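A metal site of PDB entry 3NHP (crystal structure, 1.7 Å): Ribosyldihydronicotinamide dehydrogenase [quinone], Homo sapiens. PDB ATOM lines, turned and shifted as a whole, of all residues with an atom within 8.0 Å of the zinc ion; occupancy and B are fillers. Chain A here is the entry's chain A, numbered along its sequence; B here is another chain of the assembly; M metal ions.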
ATOM      1  N   TYR A 132     -32.756 -11.239 -29.496  1.00  0.00           N
ATOM      2  CA  TYR A 132     -32.599 -10.649 -28.190  1.00  0.00           C
ATOM      3  C   TYR A 132     -33.636 -11.241 -27.199  1.00  0.00           C
ATOM      4  O   TYR A 132     -33.645 -12.484 -27.016  1.00  0.00           O
ATOM      5  CB  TYR A 132     -32.507  -9.114 -28.279  1.00  0.00           C
ATOM      6  CG  TYR A 132     -31.098  -8.774 -28.777  1.00  0.00           C
ATOM      7  CD1 TYR A 132     -29.953  -9.345 -28.160  1.00  0.00           C
ATOM      8  CD2 TYR A 132     -30.901  -7.903 -29.871  1.00  0.00           C
ATOM      9  CE1 TYR A 132     -28.659  -9.077 -28.653  1.00  0.00           C
ATOM     10  CE2 TYR A 132     -29.604  -7.624 -30.354  1.00  0.00           C
ATOM     11  CZ  TYR A 132     -28.507  -8.226 -29.753  1.00  0.00           C
ATOM     12  OH  TYR A 132     -27.272  -7.936 -30.263  1.00  0.00           O
ATOM     13  N   ASP A 133     -34.481 -10.410 -26.600  1.00  0.00           N
ATOM     14  CA  ASP A 133     -35.585 -10.890 -25.742  1.00  0.00           C
ATOM     15  C   ASP A 133     -36.545 -11.900 -26.347  1.00  0.00           C
ATOM     16  O   ASP A 133     -37.048 -12.800 -25.630  1.00  0.00           O
ATOM     17  CB  ASP A 133     -36.374  -9.701 -25.197  1.00  0.00           C
ATOM     18  CG  ASP A 133     -35.608  -8.971 -24.143  1.00  0.00           C
ATOM     19  OD1 ASP A 133     -34.429  -9.367 -23.899  1.00  0.00           O
ATOM     20  OD2 ASP A 133     -36.147  -8.022 -23.540  1.00  0.00           O
ATOM     21  N   TRP A 169     -19.044  -9.719 -23.823  1.00  0.00           N
ATOM     22  CA  TRP A 169     -20.062  -9.186 -24.714  1.00  0.00           C
ATOM     23  C   TRP A 169     -20.401  -9.933 -25.997  1.00  0.00           C
ATOM     24  O   TRP A 169     -21.619 -10.103 -26.318  1.00  0.00           O
ATOM     25  CB  TRP A 169     -19.745  -7.676 -25.036  1.00  0.00           C
ATOM     26  CG  TRP A 169     -20.602  -6.931 -26.015  1.00  0.00           C
ATOM     27  CD1 TRP A 169     -20.256  -6.511 -27.250  1.00  0.00           C
ATOM     28  CD2 TRP A 169     -21.884  -6.322 -25.755  1.00  0.00           C
ATOM     29  NE1 TRP A 169     -21.276  -5.765 -27.849  1.00  0.00           N
ATOM     30  CE2 TRP A 169     -22.264  -5.596 -26.911  1.00  0.00           C
ATOM     31  CE3 TRP A 169     -22.746  -6.320 -24.632  1.00  0.00           C
ATOM     32  CZ2 TRP A 169     -23.509  -4.928 -27.016  1.00  0.00           C
ATOM     33  CZ3 TRP A 169     -23.978  -5.645 -24.737  1.00  0.00           C
ATOM     34  CH2 TRP A 169     -24.328  -4.948 -25.903  1.00  0.00           C
ATOM     35  N   LEU A 171     -20.089 -12.962 -26.549  1.00  0.00           N
ATOM     36  CA  LEU A 171     -20.621 -14.311 -26.199  1.00  0.00           C
ATOM     37  C   LEU A 171     -21.951 -14.208 -25.459  1.00  0.00           C
ATOM     38  O   LEU A 171     -22.904 -14.731 -25.935  1.00  0.00           O
ATOM     39  CB  LEU A 171     -19.638 -15.091 -25.317  1.00  0.00           C
ATOM     40  CG  LEU A 171     -18.244 -15.255 -25.977  1.00  0.00           C
ATOM     41  CD1 LEU A 171     -17.314 -15.848 -24.993  1.00  0.00           C
ATOM     42  CD2 LEU A 171     -18.357 -16.181 -27.207  1.00  0.00           C
ATOM     43  N   GLN A 172     -21.982 -13.486 -24.369  1.00  0.00           N
ATOM     44  CA  GLN A 172     -23.223 -13.355 -23.612  1.00  0.00           C
ATOM     45  C   GLN A 172     -24.262 -12.604 -24.340  1.00  0.00           C
ATOM     46  O   GLN A 172     -25.443 -13.061 -24.455  1.00  0.00           O
ATOM     47  CB  GLN A 172     -22.938 -12.705 -22.294  1.00  0.00           C
ATOM     48  CG  GLN A 172     -22.173 -13.568 -21.382  1.00  0.00           C
ATOM     49  CD  GLN A 172     -22.238 -13.007 -20.011  1.00  0.00           C
ATOM     50  OE1 GLN A 172     -22.397 -11.768 -19.807  1.00  0.00           O
ATOM     51  NE2 GLN A 172     -21.988 -13.870 -19.039  1.00  0.00           N
ATOM     52  N   HIS A 173     -23.889 -11.413 -24.853  1.00  0.00           N
ATOM     53  CA  HIS A 173     -24.887 -10.587 -25.568  1.00  0.00           C
ATOM     54  C   HIS A 173     -25.047 -10.893 -27.011  1.00  0.00           C
ATOM     55  O   HIS A 173     -26.152 -11.194 -27.481  1.00  0.00           O
ATOM     56  CB  HIS A 173     -24.553  -9.103 -25.429  1.00  0.00           C
ATOM     57  CG  HIS A 173     -25.595  -8.203 -26.040  1.00  0.00           C
ATOM     58  ND1 HIS A 173     -26.801  -7.955 -25.421  1.00  0.00           N
ATOM     59  CD2 HIS A 173     -25.622  -7.516 -27.207  1.00  0.00           C
ATOM     60  CE1 HIS A 173     -27.524  -7.141 -26.175  1.00  0.00           C
ATOM     61  NE2 HIS A 173     -26.818  -6.850 -27.260  1.00  0.00           N
ATOM     62  N   GLY A 174     -23.947 -10.841 -27.765  1.00  0.00           N
ATOM     63  CA  GLY A 174     -24.066 -11.009 -29.210  1.00  0.00           C
ATOM     64  C   GLY A 174     -24.499 -12.429 -29.614  1.00  0.00           C
ATOM     65  O   GLY A 174     -25.021 -12.592 -30.676  1.00  0.00           O
ATOM     66  N   THR A 175     -24.281 -13.418 -28.741  1.00  0.00           N
ATOM     67  CA  THR A 175     -24.620 -14.820 -29.161  1.00  0.00           C
ATOM     68  C   THR A 175     -25.820 -15.315 -28.301  1.00  0.00           C
ATOM     69  O   THR A 175     -26.888 -15.564 -28.837  1.00  0.00           O
ATOM     70  CB  THR A 175     -23.398 -15.708 -28.980  1.00  0.00           C
ATOM     71  OG1 THR A 175     -22.326 -15.194 -29.811  1.00  0.00           O
ATOM     72  CG2 THR A 175     -23.703 -17.068 -29.445  1.00  0.00           C
ATOM     73  N   LEU A 176     -25.594 -15.437 -27.019  1.00  0.00           N
ATOM     74  CA  LEU A 176     -26.596 -16.116 -26.104  1.00  0.00           C
ATOM     75  C   LEU A 176     -27.888 -15.304 -25.957  1.00  0.00           C
ATOM     76  O   LEU A 176     -28.984 -15.792 -26.289  1.00  0.00           O
ATOM     77  CB  LEU A 176     -25.979 -16.446 -24.747  1.00  0.00           C
ATOM     78  CG  LEU A 176     -24.728 -17.394 -24.819  1.00  0.00           C
ATOM     79  CD1 LEU A 176     -24.078 -17.510 -23.503  1.00  0.00           C
ATOM     80  CD2 LEU A 176     -25.031 -18.779 -25.503  1.00  0.00           C
ATOM     81  N   HIS A 177     -27.746 -14.016 -25.641  1.00  0.00           N
ATOM     82  CA  HIS A 177     -28.946 -13.118 -25.551  1.00  0.00           C
ATOM     83  C   HIS A 177     -29.669 -12.987 -26.884  1.00  0.00           C
ATOM     84  O   HIS A 177     -30.907 -13.081 -26.994  1.00  0.00           O
ATOM     85  CB  HIS A 177     -28.537 -11.743 -24.964  1.00  0.00           C
ATOM     86  CG  HIS A 177     -29.709 -10.851 -24.652  1.00  0.00           C
ATOM     87  ND1 HIS A 177     -29.545  -9.630 -24.003  1.00  0.00           N
ATOM     88  CD2 HIS A 177     -31.036 -11.020 -24.812  1.00  0.00           C
ATOM     89  CE1 HIS A 177     -30.732  -9.070 -23.848  1.00  0.00           C
ATOM     90  NE2 HIS A 177     -31.663  -9.901 -24.304  1.00  0.00           N
ATOM     91  N   PHE A 178     -28.906 -12.791 -27.947  1.00  0.00           N
ATOM     92  CA  PHE A 178     -29.468 -12.788 -29.243  1.00  0.00           C
ATOM     93  C   PHE A 178     -30.319 -13.976 -29.538  1.00  0.00           C
ATOM     94  O   PHE A 178     -31.323 -13.824 -30.221  1.00  0.00           O
ATOM     95  CB  PHE A 178     -28.361 -12.600 -30.317  1.00  0.00           C
ATOM     96  CG  PHE A 178     -28.895 -12.372 -31.695  1.00  0.00           C
ATOM     97  CD1 PHE A 178     -29.161 -11.046 -32.152  1.00  0.00           C
ATOM     98  CD2 PHE A 178     -29.137 -13.411 -32.539  1.00  0.00           C
ATOM     99  CE1 PHE A 178     -29.679 -10.848 -33.480  1.00  0.00           C
ATOM    100  CE2 PHE A 178     -29.679 -13.259 -33.831  1.00  0.00           C
ATOM    101  CZ  PHE A 178     -29.928 -11.950 -34.317  1.00  0.00           C
ATOM    102  N   PHE A 181     -31.648 -16.702 -24.927  1.00  0.00           N
ATOM    103  CA  PHE A 181     -31.235 -17.148 -23.606  1.00  0.00           C
ATOM    104  C   PHE A 181     -31.335 -16.103 -22.548  1.00  0.00           C
ATOM    105  O   PHE A 181     -31.059 -14.932 -22.775  1.00  0.00           O
ATOM    106  CB  PHE A 181     -29.776 -17.661 -23.617  1.00  0.00           C
ATOM    107  CG  PHE A 181     -29.582 -19.010 -24.321  1.00  0.00           C
ATOM    108  CD1 PHE A 181     -29.976 -20.205 -23.710  1.00  0.00           C
ATOM    109  CD2 PHE A 181     -28.876 -19.095 -25.509  1.00  0.00           C
ATOM    110  CE1 PHE A 181     -29.728 -21.455 -24.345  1.00  0.00           C
ATOM    111  CE2 PHE A 181     -28.650 -20.303 -26.161  1.00  0.00           C
ATOM    112  CZ  PHE A 181     -29.081 -21.518 -25.550  1.00  0.00           C
ATOM    113  N   VAL A 183     -29.218 -15.275 -19.449  1.00  0.00           N
ATOM    114  CA  VAL A 183     -27.849 -15.514 -19.207  1.00  0.00           C
ATOM    115  C   VAL A 183     -27.606 -15.417 -17.744  1.00  0.00           C
ATOM    116  O   VAL A 183     -27.751 -14.340 -17.133  1.00  0.00           O
ATOM    117  CB  VAL A 183     -26.886 -14.489 -19.954  1.00  0.00           C
ATOM    118  CG1 VAL A 183     -25.425 -14.862 -19.735  1.00  0.00           C
ATOM    119  CG2 VAL A 183     -27.175 -14.463 -21.368  1.00  0.00           C
ATOM    120  N   ILE A 220     -28.627 -12.313 -15.243  1.00  0.00           N
ATOM    121  CA  ILE A 220     -28.075 -10.965 -15.289  1.00  0.00           C
ATOM    122  C   ILE A 220     -28.905 -10.115 -16.262  1.00  0.00           C
ATOM    123  O   ILE A 220     -29.586 -10.633 -17.145  1.00  0.00           O
ATOM    124  CB  ILE A 220     -26.581 -11.026 -15.740  1.00  0.00           C
ATOM    125  CG1 ILE A 220     -26.439 -11.567 -17.168  1.00  0.00           C
ATOM    126  CG2 ILE A 220     -25.765 -11.800 -14.696  1.00  0.00           C
ATOM    127  CD1 ILE A 220     -25.181 -11.060 -17.856  1.00  0.00           C
ATOM    128  N   PRO A 221     -28.918  -8.774 -16.075  1.00  0.00           N
ATOM    129  CA  PRO A 221     -29.504  -7.985 -17.130  1.00  0.00           C
ATOM    130  C   PRO A 221     -28.444  -7.921 -18.183  1.00  0.00           C
ATOM    131  O   PRO A 221     -27.356  -7.388 -17.898  1.00  0.00           O
ATOM    132  CB  PRO A 221     -29.652  -6.574 -16.521  1.00  0.00           C
ATOM    133  CG  PRO A 221     -28.732  -6.535 -15.379  1.00  0.00           C
ATOM    134  CD  PRO A 221     -28.632  -7.987 -14.863  1.00  0.00           C
ATOM    135  N   CYS A 222     -28.744  -8.478 -19.374  1.00  0.00           N
ATOM    136  CA  CYS A 222     -27.732  -8.648 -20.425  1.00  0.00           C
ATOM    137  C   CYS A 222     -27.762  -7.421 -21.347  1.00  0.00           C
ATOM    138  O   CYS A 222     -28.304  -7.422 -22.441  1.00  0.00           O
ATOM    139  CB  CYS A 222     -27.881  -9.979 -21.182  1.00  0.00           C
ATOM    140  SG  CYS A 222     -26.506 -10.225 -22.408  1.00  0.00           S
ATOM    141  N   THR A 223     -27.203  -6.342 -20.835  1.00  0.00           N
ATOM    142  CA  THR A 223     -27.293  -5.085 -21.536  1.00  0.00           C
ATOM    143  C   THR A 223     -25.909  -4.471 -21.674  1.00  0.00           C
ATOM    144  O   THR A 223     -24.945  -4.855 -20.982  1.00  0.00           O
ATOM    145  CB  THR A 223     -28.198  -4.083 -20.720  1.00  0.00           C
ATOM    146  OG1 THR A 223     -27.638  -3.927 -19.416  1.00  0.00           O
ATOM    147  CG2 THR A 223     -29.680  -4.569 -20.628  1.00  0.00           C
ATOM    148  N   ALA A 224     -25.841  -3.451 -22.518  1.00  0.00           N
ATOM    149  CA  ALA A 224     -24.605  -2.685 -22.680  1.00  0.00           C
ATOM    150  C   ALA A 224     -24.165  -2.104 -21.333  1.00  0.00           C
ATOM    151  O   ALA A 224     -23.001  -2.218 -20.933  1.00  0.00           O
ATOM    152  CB  ALA A 224     -24.794  -1.585 -23.758  1.00  0.00           C
ATOM    153  N   TRP A 226     -24.701  -3.315 -18.261  1.00  0.00           N
ATOM    154  CA  TRP A 226     -24.064  -4.336 -17.429  1.00  0.00           C
ATOM    155  C   TRP A 226     -22.614  -4.590 -17.890  1.00  0.00           C
ATOM    156  O   TRP A 226     -21.719  -4.776 -17.083  1.00  0.00           O
ATOM    157  CB  TRP A 226     -24.892  -5.655 -17.406  1.00  0.00           C
ATOM    158  CG  TRP A 226     -24.377  -6.729 -16.445  1.00  0.00           C
ATOM    159  CD1 TRP A 226     -24.746  -6.929 -15.133  1.00  0.00           C
ATOM    160  CD2 TRP A 226     -23.388  -7.729 -16.744  1.00  0.00           C
ATOM    161  NE1 TRP A 226     -24.070  -7.999 -14.610  1.00  0.00           N
ATOM    162  CE2 TRP A 226     -23.217  -8.511 -15.560  1.00  0.00           C
ATOM    163  CE3 TRP A 226     -22.615  -8.040 -17.878  1.00  0.00           C
ATOM    164  CZ2 TRP A 226     -22.308  -9.581 -15.492  1.00  0.00           C
ATOM    165  CZ3 TRP A 226     -21.692  -9.120 -17.792  1.00  0.00           C
ATOM    166  CH2 TRP A 226     -21.548  -9.866 -16.618  1.00  0.00           C
ATOM    167  N   HIS A 227     -22.378  -4.582 -19.208  1.00  0.00           N
ATOM    168  CA  HIS A 227     -21.041  -4.959 -19.683  1.00  0.00           C
ATOM    169  C   HIS A 227     -20.025  -3.805 -19.615  1.00  0.00           C
ATOM    170  O   HIS A 227     -18.830  -4.028 -19.414  1.00  0.00           O
ATOM    171  CB  HIS A 227     -21.120  -5.519 -21.109  1.00  0.00           C
ATOM    172  CG  HIS A 227     -21.737  -6.896 -21.193  1.00  0.00           C
ATOM    173  ND1 HIS A 227     -23.102  -7.101 -21.335  1.00  0.00           N
ATOM    174  CD2 HIS A 227     -21.168  -8.127 -21.200  1.00  0.00           C
ATOM    175  CE1 HIS A 227     -23.345  -8.405 -21.422  1.00  0.00           C
ATOM    176  NE2 HIS A 227     -22.180  -9.040 -21.328  1.00  0.00           N
ATOM    177  N   VAL B 160     -29.223  -1.691 -31.073  1.00  0.00           N
ATOM    178  CA  VAL B 160     -29.484  -2.989 -30.401  1.00  0.00           C
ATOM    179  C   VAL B 160     -28.249  -3.824 -30.144  1.00  0.00           C
ATOM    180  O   VAL B 160     -28.102  -4.529 -29.100  1.00  0.00           O
ATOM    181  CB  VAL B 160     -30.452  -3.848 -31.211  1.00  0.00           C
ATOM    182  CG1 VAL B 160     -31.839  -3.699 -30.644  1.00  0.00           C
ATOM    183  CG2 VAL B 160     -30.360  -3.528 -32.729  1.00  0.00           C
HETATM  184 ZN    ZN M   1     -27.671  -8.898 -23.832  1.00  0.00          ZN
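Residues that only touch the zinc ion: Thr 223 (3.97 Å).
Along chain A the residues within 4 Å of the zinc ion span positions 173 to 223.
The nearest printed residue that does not touch the zinc ion is Gln 172 (4.8 Å).
N of Trp 226 sits at hydrogen-bond distance from OG1 of Thr 223, 3.2 Å away.
NE2 of His 173 lies within hydrogen-bond range of O of Val 160 of chain B.
O of His 173 lies within hydrogen-bond range of N of Phe 178 (3.2 Å).
O of Thr 223 lies within hydrogen-bond range of ND1 of His 227 (2.9 Å).
NE2 of His 173 sits close to OH of Tyr 132.
NE2 of His 177 sits at hydrogen-bond distance from OD1 of Asp 133 (2.8 Å).
The backbone carbonyl oxygen (O) of Gln 172 sits close to the side-chain sulfur (SG) of Cys 222, 3.7 Å away.
The backbone carbonyl oxygen (O) of Gln 172 sits at hydrogen-bond distance from the backbone NH (N) of His 177, at 2.8 Å.
The zinc ion is bound by a ring nitrogen (ND1) of His 177, a ring nitrogen (ND1) of His 173, the backbone carbonyl oxygen of Cys 222 and the side-chain sulfur of Cys 222.
The zinc ion has four donor atoms within binding distance.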
